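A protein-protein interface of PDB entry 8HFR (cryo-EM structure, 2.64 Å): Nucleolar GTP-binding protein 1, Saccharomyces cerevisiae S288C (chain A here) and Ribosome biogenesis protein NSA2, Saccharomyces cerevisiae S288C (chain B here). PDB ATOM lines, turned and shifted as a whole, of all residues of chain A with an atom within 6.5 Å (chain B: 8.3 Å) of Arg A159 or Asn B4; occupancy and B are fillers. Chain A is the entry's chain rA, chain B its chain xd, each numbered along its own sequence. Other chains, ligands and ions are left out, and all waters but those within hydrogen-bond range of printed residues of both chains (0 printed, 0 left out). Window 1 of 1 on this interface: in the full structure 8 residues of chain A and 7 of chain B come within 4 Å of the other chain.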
ATOM      1  N   TRP A   5     -17.768   8.937  24.436  1.00  0.00           N
ATOM      2  CA  TRP A   5     -18.153   7.905  25.391  1.00  0.00           C
ATOM      3  C   TRP A   5     -17.997   8.401  26.821  1.00  0.00           C
ATOM      4  O   TRP A   5     -17.427   7.731  27.683  1.00  0.00           O
ATOM      5  CB  TRP A   5     -17.343   6.639  25.155  1.00  0.00           C
ATOM      6  CG  TRP A   5     -17.612   6.047  23.820  1.00  0.00           C
ATOM      7  CD1 TRP A   5     -18.635   5.217  23.487  1.00  0.00           C
ATOM      8  CD2 TRP A   5     -16.857   6.256  22.622  1.00  0.00           C
ATOM      9  NE1 TRP A   5     -18.562   4.888  22.157  1.00  0.00           N
ATOM     10  CE2 TRP A   5     -17.477   5.514  21.605  1.00  0.00           C
ATOM     11  CE3 TRP A   5     -15.712   6.994  22.316  1.00  0.00           C
ATOM     12  CZ2 TRP A   5     -16.995   5.488  20.306  1.00  0.00           C
ATOM     13  CZ3 TRP A   5     -15.237   6.970  21.025  1.00  0.00           C
ATOM     14  CH2 TRP A   5     -15.874   6.221  20.035  1.00  0.00           C
ATOM     15  N   LYS A   6     -18.501   9.600  27.092  1.00  0.00           N
ATOM     16  CA  LYS A   6     -18.659  10.068  28.468  1.00  0.00           C
ATOM     17  C   LYS A   6     -20.062   9.765  28.988  1.00  0.00           C
ATOM     18  O   LYS A   6     -20.767  10.637  29.487  1.00  0.00           O
ATOM     19  CB  LYS A   6     -18.352  11.555  28.552  1.00  0.00           C
ATOM     20  CG  LYS A   6     -17.793  12.000  29.885  1.00  0.00           C
ATOM     21  CD  LYS A   6     -17.743  13.505  29.970  1.00  0.00           C
ATOM     22  CE  LYS A   6     -17.676  13.970  31.396  1.00  0.00           C
ATOM     23  NZ  LYS A   6     -17.610  15.443  31.455  1.00  0.00           N
ATOM     24  N   ARG A 154     -12.250   3.000  31.391  1.00  0.00           N
ATOM     25  CA  ARG A 154     -13.371   3.937  31.371  1.00  0.00           C
ATOM     26  C   ARG A 154     -12.910   5.344  31.716  1.00  0.00           C
ATOM     27  O   ARG A 154     -13.295   6.323  31.052  1.00  0.00           O
ATOM     28  CB  ARG A 154     -14.462   3.492  32.340  1.00  0.00           C
ATOM     29  CG  ARG A 154     -15.635   4.452  32.382  1.00  0.00           C
ATOM     30  CD  ARG A 154     -16.330   4.435  33.714  1.00  0.00           C
ATOM     31  NE  ARG A 154     -15.514   5.014  34.769  1.00  0.00           N
ATOM     32  CZ  ARG A 154     -15.786   6.165  35.364  1.00  0.00           C
ATOM     33  NH1 ARG A 154     -16.850   6.858  34.999  1.00  0.00           N
ATOM     34  NH2 ARG A 154     -14.995   6.622  36.322  1.00  0.00           N
ATOM     35  N   GLN A 155     -12.066   5.454  32.751  1.00  0.00           N
ATOM     36  CA  GLN A 155     -11.510   6.745  33.140  1.00  0.00           C
ATOM     37  C   GLN A 155     -10.686   7.368  32.019  1.00  0.00           C
ATOM     38  O   GLN A 155     -10.683   8.593  31.855  1.00  0.00           O
ATOM     39  CB  GLN A 155     -10.649   6.575  34.386  1.00  0.00           C
ATOM     40  CG  GLN A 155     -11.409   6.493  35.677  1.00  0.00           C
ATOM     41  CD  GLN A 155     -10.570   6.963  36.837  1.00  0.00           C
ATOM     42  OE1 GLN A 155      -9.535   7.594  36.645  1.00  0.00           O
ATOM     43  NE2 GLN A 155     -11.004   6.657  38.047  1.00  0.00           N
ATOM     44  N   HIS A 156      -9.995   6.544  31.225  1.00  0.00           N
ATOM     45  CA  HIS A 156      -9.232   7.101  30.112  1.00  0.00           C
ATOM     46  C   HIS A 156     -10.124   7.441  28.921  1.00  0.00           C
ATOM     47  O   HIS A 156      -9.918   8.467  28.265  1.00  0.00           O
ATOM     48  CB  HIS A 156      -8.128   6.142  29.684  1.00  0.00           C
ATOM     49  CG  HIS A 156      -7.365   6.607  28.485  1.00  0.00           C
ATOM     50  ND1 HIS A 156      -6.312   7.489  28.574  1.00  0.00           N
ATOM     51  CD2 HIS A 156      -7.506   6.320  27.170  1.00  0.00           C
ATOM     52  CE1 HIS A 156      -5.837   7.725  27.365  1.00  0.00           C
ATOM     53  NE2 HIS A 156      -6.546   7.031  26.495  1.00  0.00           N
ATOM     54  N   ILE A 157     -11.113   6.596  28.615  1.00  0.00           N
ATOM     55  CA  ILE A 157     -11.908   6.789  27.409  1.00  0.00           C
ATOM     56  C   ILE A 157     -12.912   7.923  27.563  1.00  0.00           C
ATOM     57  O   ILE A 157     -13.439   8.412  26.559  1.00  0.00           O
ATOM     58  CB  ILE A 157     -12.601   5.463  27.021  1.00  0.00           C
ATOM     59  CG1 ILE A 157     -12.812   5.370  25.515  1.00  0.00           C
ATOM     60  CG2 ILE A 157     -13.930   5.286  27.729  1.00  0.00           C
ATOM     61  CD1 ILE A 157     -11.548   5.110  24.749  1.00  0.00           C
ATOM     62  N   GLY A 158     -13.195   8.361  28.794  1.00  0.00           N
ATOM     63  CA  GLY A 158     -14.104   9.483  28.962  1.00  0.00           C
ATOM     64  C   GLY A 158     -13.552  10.805  28.464  1.00  0.00           C
ATOM     65  O   GLY A 158     -14.308  11.653  27.986  1.00  0.00           O
ATOM     66  N   ARG A 159     -12.234  11.000  28.560  1.00  0.00           N
ATOM     67  CA  ARG A 159     -11.598  12.261  28.191  1.00  0.00           C
ATOM     68  C   ARG A 159     -11.317  12.395  26.703  1.00  0.00           C
ATOM     69  O   ARG A 159     -10.836  13.447  26.281  1.00  0.00           O
ATOM     70  CB  ARG A 159     -10.266  12.442  28.922  1.00  0.00           C
ATOM     71  CG  ARG A 159     -10.330  12.956  30.335  1.00  0.00           C
ATOM     72  CD  ARG A 159     -10.420  11.840  31.321  1.00  0.00           C
ATOM     73  NE  ARG A 159      -9.338  10.882  31.122  1.00  0.00           N
ATOM     74  CZ  ARG A 159      -8.115  11.009  31.619  1.00  0.00           C
ATOM     75  NH1 ARG A 159      -7.806  12.053  32.356  1.00  0.00           N
ATOM     76  NH2 ARG A 159      -7.203  10.085  31.378  1.00  0.00           N
ATOM     77  N   LEU A 160     -11.599  11.375  25.913  1.00  0.00           N
ATOM     78  CA  LEU A 160     -11.049  11.286  24.571  1.00  0.00           C
ATOM     79  C   LEU A 160     -11.783  12.234  23.623  1.00  0.00           C
ATOM     80  O   LEU A 160     -12.998  12.411  23.745  1.00  0.00           O
ATOM     81  CB  LEU A 160     -11.153   9.843  24.093  1.00  0.00           C
ATOM     82  CG  LEU A 160     -10.363   9.350  22.894  1.00  0.00           C
ATOM     83  CD1 LEU A 160      -9.718   8.068  23.281  1.00  0.00           C
ATOM     84  CD2 LEU A 160     -11.290   9.124  21.723  1.00  0.00           C
ATOM     85  N   PRO A 161     -11.072  12.878  22.693  1.00  0.00           N
ATOM     86  CA  PRO A 161     -11.707  13.865  21.811  1.00  0.00           C
ATOM     87  C   PRO A 161     -12.681  13.229  20.839  1.00  0.00           C
ATOM     88  O   PRO A 161     -12.720  12.015  20.635  1.00  0.00           O
ATOM     89  CB  PRO A 161     -10.530  14.494  21.068  1.00  0.00           C
ATOM     90  CG  PRO A 161      -9.365  14.216  21.900  1.00  0.00           C
ATOM     91  CD  PRO A 161      -9.609  12.913  22.561  1.00  0.00           C
ATOM     92  N   SER A 203      -0.505  12.551  22.439  1.00  0.00           N
ATOM     93  CA  SER A 203      -1.810  12.151  21.939  1.00  0.00           C
ATOM     94  C   SER A 203      -2.169  13.075  20.782  1.00  0.00           C
ATOM     95  O   SER A 203      -1.336  13.850  20.306  1.00  0.00           O
ATOM     96  CB  SER A 203      -2.844  12.170  23.068  1.00  0.00           C
ATOM     97  OG  SER A 203      -2.938  13.454  23.640  1.00  0.00           O
ATOM     98  N   LEU A 204      -3.410  12.994  20.320  1.00  0.00           N
ATOM     99  CA  LEU A 204      -3.863  13.760  19.167  1.00  0.00           C
ATOM    100  C   LEU A 204      -5.004  14.682  19.573  1.00  0.00           C
ATOM    101  O   LEU A 204      -5.874  14.296  20.354  1.00  0.00           O
ATOM    102  CB  LEU A 204      -4.276  12.830  18.014  1.00  0.00           C
ATOM    103  CG  LEU A 204      -5.575  12.019  17.944  1.00  0.00           C
ATOM    104  CD1 LEU A 204      -5.739  11.445  16.552  1.00  0.00           C
ATOM    105  CD2 LEU A 204      -5.615  10.894  18.959  1.00  0.00           C
ATOM    106  N   TYR A 205      -4.980  15.909  19.054  1.00  0.00           N
ATOM    107  CA  TYR A 205      -5.880  16.972  19.473  1.00  0.00           C
ATOM    108  C   TYR A 205      -6.695  17.472  18.292  1.00  0.00           C
ATOM    109  O   TYR A 205      -6.277  17.368  17.139  1.00  0.00           O
ATOM    110  CB  TYR A 205      -5.116  18.149  20.089  1.00  0.00           C
ATOM    111  CG  TYR A 205      -4.439  17.844  21.405  1.00  0.00           C
ATOM    112  CD1 TYR A 205      -3.209  17.197  21.446  1.00  0.00           C
ATOM    113  CD2 TYR A 205      -5.020  18.221  22.608  1.00  0.00           C
ATOM    114  CE1 TYR A 205      -2.588  16.917  22.641  1.00  0.00           C
ATOM    115  CE2 TYR A 205      -4.403  17.948  23.812  1.00  0.00           C
ATOM    116  CZ  TYR A 205      -3.188  17.294  23.821  1.00  0.00           C
ATOM    117  OH  TYR A 205      -2.566  17.018  25.017  1.00  0.00           O
ATOM    118  N   GLN A 238      -1.046   5.832  16.601  1.00  0.00           N
ATOM    119  CA  GLN A 238      -2.165   6.777  16.560  1.00  0.00           C
ATOM    120  C   GLN A 238      -2.108   7.659  15.319  1.00  0.00           C
ATOM    121  O   GLN A 238      -3.103   7.806  14.598  1.00  0.00           O
ATOM    122  CB  GLN A 238      -2.160   7.647  17.819  1.00  0.00           C
ATOM    123  CG  GLN A 238      -2.653   6.944  19.069  1.00  0.00           C
ATOM    124  CD  GLN A 238      -2.625   7.841  20.285  1.00  0.00           C
ATOM    125  OE1 GLN A 238      -3.367   8.815  20.365  1.00  0.00           O
ATOM    126  NE2 GLN A 238      -1.762   7.518  21.240  1.00  0.00           N
ATOM    127  N   PRO B   2     -13.344  19.694  26.700  1.00  0.00           N
ATOM    128  CA  PRO B   2     -11.938  19.443  26.990  1.00  0.00           C
ATOM    129  C   PRO B   2     -11.498  18.083  26.461  1.00  0.00           C
ATOM    130  O   PRO B   2     -12.190  17.078  26.577  1.00  0.00           O
ATOM    131  CB  PRO B   2     -11.885  19.521  28.508  1.00  0.00           C
ATOM    132  CG  PRO B   2     -13.201  19.115  28.942  1.00  0.00           C
ATOM    133  CD  PRO B   2     -14.176  19.538  27.894  1.00  0.00           C
ATOM    134  N   GLN B   3     -10.334  18.102  25.827  1.00  0.00           N
ATOM    135  CA  GLN B   3      -9.724  16.977  25.131  1.00  0.00           C
ATOM    136  C   GLN B   3      -9.045  16.034  26.105  1.00  0.00           C
ATOM    137  O   GLN B   3      -9.478  15.903  27.249  1.00  0.00           O
ATOM    138  CB  GLN B   3      -8.722  17.472  24.095  1.00  0.00           C
ATOM    139  CG  GLN B   3      -9.341  17.901  22.804  1.00  0.00           C
ATOM    140  CD  GLN B   3      -8.741  19.183  22.313  1.00  0.00           C
ATOM    141  OE1 GLN B   3      -7.914  19.786  22.988  1.00  0.00           O
ATOM    142  NE2 GLN B   3      -9.165  19.624  21.146  1.00  0.00           N
ATOM    143  N   ASN B   4      -8.050  15.298  25.610  1.00  0.00           N
ATOM    144  CA  ASN B   4      -7.108  14.492  26.385  1.00  0.00           C
ATOM    145  C   ASN B   4      -6.597  15.219  27.626  1.00  0.00           C
ATOM    146  O   ASN B   4      -6.466  16.449  27.596  1.00  0.00           O
ATOM    147  CB  ASN B   4      -5.928  14.131  25.493  1.00  0.00           C
ATOM    148  CG  ASN B   4      -6.326  13.251  24.340  1.00  0.00           C
ATOM    149  OD1 ASN B   4      -6.988  12.232  24.519  1.00  0.00           O
ATOM    150  ND2 ASN B   4      -5.967  13.667  23.135  1.00  0.00           N
ATOM    151  N   ASP B   5      -6.195  14.444  28.645  1.00  0.00           N
ATOM    152  CA  ASP B   5      -6.249  14.740  30.080  1.00  0.00           C
ATOM    153  C   ASP B   5      -5.890  16.172  30.439  1.00  0.00           C
ATOM    154  O   ASP B   5      -4.762  16.621  30.223  1.00  0.00           O
ATOM    155  CB  ASP B   5      -5.308  13.783  30.811  1.00  0.00           C
ATOM    156  N   TYR B   6      -6.855  16.873  31.030  1.00  0.00           N
ATOM    157  CA  TYR B   6      -6.884  18.324  31.063  1.00  0.00           C
ATOM    158  C   TYR B   6      -6.793  18.912  32.455  1.00  0.00           C
ATOM    159  O   TYR B   6      -6.409  20.078  32.583  1.00  0.00           O
ATOM    160  CB  TYR B   6      -8.168  18.848  30.395  1.00  0.00           C
ATOM    161  CG  TYR B   6      -9.447  18.148  30.819  1.00  0.00           C
ATOM    162  CD1 TYR B   6     -10.186  18.597  31.911  1.00  0.00           C
ATOM    163  CD2 TYR B   6      -9.928  17.056  30.116  1.00  0.00           C
ATOM    164  CE1 TYR B   6     -11.351  17.957  32.294  1.00  0.00           C
ATOM    165  CE2 TYR B   6     -11.089  16.424  30.482  1.00  0.00           C
ATOM    166  CZ  TYR B   6     -11.795  16.869  31.573  1.00  0.00           C
ATOM    167  OH  TYR B   6     -12.954  16.225  31.931  1.00  0.00           O
ATOM    168  N   ILE B   7      -7.127  18.146  33.493  1.00  0.00           N
ATOM    169  CA  ILE B   7      -7.067  18.661  34.854  1.00  0.00           C
ATOM    170  C   ILE B   7      -5.618  18.858  35.283  1.00  0.00           C
ATOM    171  O   ILE B   7      -5.275  19.871  35.904  1.00  0.00           O
ATOM    172  CB  ILE B   7      -7.850  17.724  35.794  1.00  0.00           C
ATOM    173  CG1 ILE B   7      -9.348  18.006  35.675  1.00  0.00           C
ATOM    174  CG2 ILE B   7      -7.402  17.851  37.247  1.00  0.00           C
ATOM    175  CD1 ILE B   7      -9.729  19.391  36.121  1.00  0.00           C
ATOM    176  N   GLU B   8      -4.730  17.940  34.898  1.00  0.00           N
ATOM    177  CA  GLU B   8      -3.329  18.118  35.260  1.00  0.00           C
ATOM    178  C   GLU B   8      -2.663  19.177  34.395  1.00  0.00           C
ATOM    179  O   GLU B   8      -1.717  19.833  34.845  1.00  0.00           O
ATOM    180  CB  GLU B   8      -2.587  16.781  35.192  1.00  0.00           C
ATOM    181  CG  GLU B   8      -1.839  16.481  33.913  1.00  0.00           C
ATOM    182  CD  GLU B   8      -2.686  15.760  32.889  1.00  0.00           C
ATOM    183  OE1 GLU B   8      -3.926  15.862  32.965  1.00  0.00           O
ATOM    184  OE2 GLU B   8      -2.107  15.081  32.013  1.00  0.00           O
ATOM    185  N   ARG B   9      -3.184  19.418  33.190  1.00  0.00           N
ATOM    186  CA  ARG B   9      -2.686  20.531  32.391  1.00  0.00           C
ATOM    187  C   ARG B   9      -3.126  21.865  32.978  1.00  0.00           C
ATOM    188  O   ARG B   9      -2.355  22.831  32.981  1.00  0.00           O
ATOM    189  CB  ARG B   9      -3.163  20.394  30.951  1.00  0.00           C
ATOM    190  CG  ARG B   9      -2.161  19.747  30.032  1.00  0.00           C
ATOM    191  CD  ARG B   9      -2.434  20.130  28.588  1.00  0.00           C
ATOM    192  NE  ARG B   9      -3.861  20.180  28.284  1.00  0.00           N
ATOM    193  CZ  ARG B   9      -4.580  19.131  27.899  1.00  0.00           C
ATOM    194  NH1 ARG B   9      -4.004  17.944  27.775  1.00  0.00           N
ATOM    195  NH2 ARG B   9      -5.875  19.269  27.644  1.00  0.00           N
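The backbone carbonyl oxygen of Arg A159 sits at hydrogen-bond distance from the backbone NH of Asn B4, 3.4 Å away. The side-chain hydroxyl of Ser A203 is in hydrogen-bond range of the side-chain amide nitrogen of Asn B4 (3.1 Å). The backbone carbonyl oxygen (O) of Leu A204 is in hydrogen-bond range of the side-chain amide nitrogen (ND2) of Asn B4 (2.9 Å). The side-chain hydroxyl (OH) of Tyr A205 lies within hydrogen-bond range of the guanidinium group (NH1) of Arg B9 (3.2 Å). O of Arg A159 sits close to O of Gln B3 (3.0 Å).
The backbone carbonyl oxygen of Gln A155 is in hydrogen-bond range of the guanidinium group of Arg A159. The backbone carbonyl oxygen (O) of Asn B4 sits at hydrogen-bond distance from the guanidinium group (NH2) of Arg B9, 2.9 Å away. The guanidinium group (NH1) of Arg B9 lies within hydrogen-bond range of the backbone carbonyl oxygen (O) of Asp B5 (2.9 Å).
Among the printed residues, merely in contact across the chains: Tyr A205 with Gln B3 (3.3 Å), Pro A161 with Asn B4 (3.3 Å), Arg A159 with Asp B5 (3.4 Å), Arg A159 with Tyr B6 (3.6 Å), Pro A161 with Gln B3 (3.8 Å) and Arg A159 with Pro B2 (3.9 Å).
Of chain B, only Pro B2 (3.9 Å), Gln B3 (3.0 Å), Asn B4 (3.4 Å), Asp B5 (3.4 Å) and Tyr B6 (3.6 Å) come within 4 Å of Arg A159. Asn B4 touches just these residues of chain A: Arg A159 (3.4 Å), Pro A161 (3.3 Å), Ser A203 (3.1 Å) and Leu A204 (2.9 Å). Of the printed residues of chain A, Gln B3 touches Arg A159, Pro A161 and Tyr A205. Of the printed residues of chain B, Pro A161 touches Gln B3 (3.8 Å) and Asn B4 (3.3 Å). His A156 touches none of the printed residues of chain B. The nearest printed residue of chain B that does not touch Pro A161 is Pro B2 (5.8 Å).
Of the 8 printed residues of chain B, 6 touch a printed residue of chain A. Hydrophobic or aromatic side chains of chain B that line the printed part of chain A: Tyr B6. Among the printed residues, no Asp or Glu carboxylate lies within 4 Å of a Lys or Arg side-chain nitrogen of the other chain.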
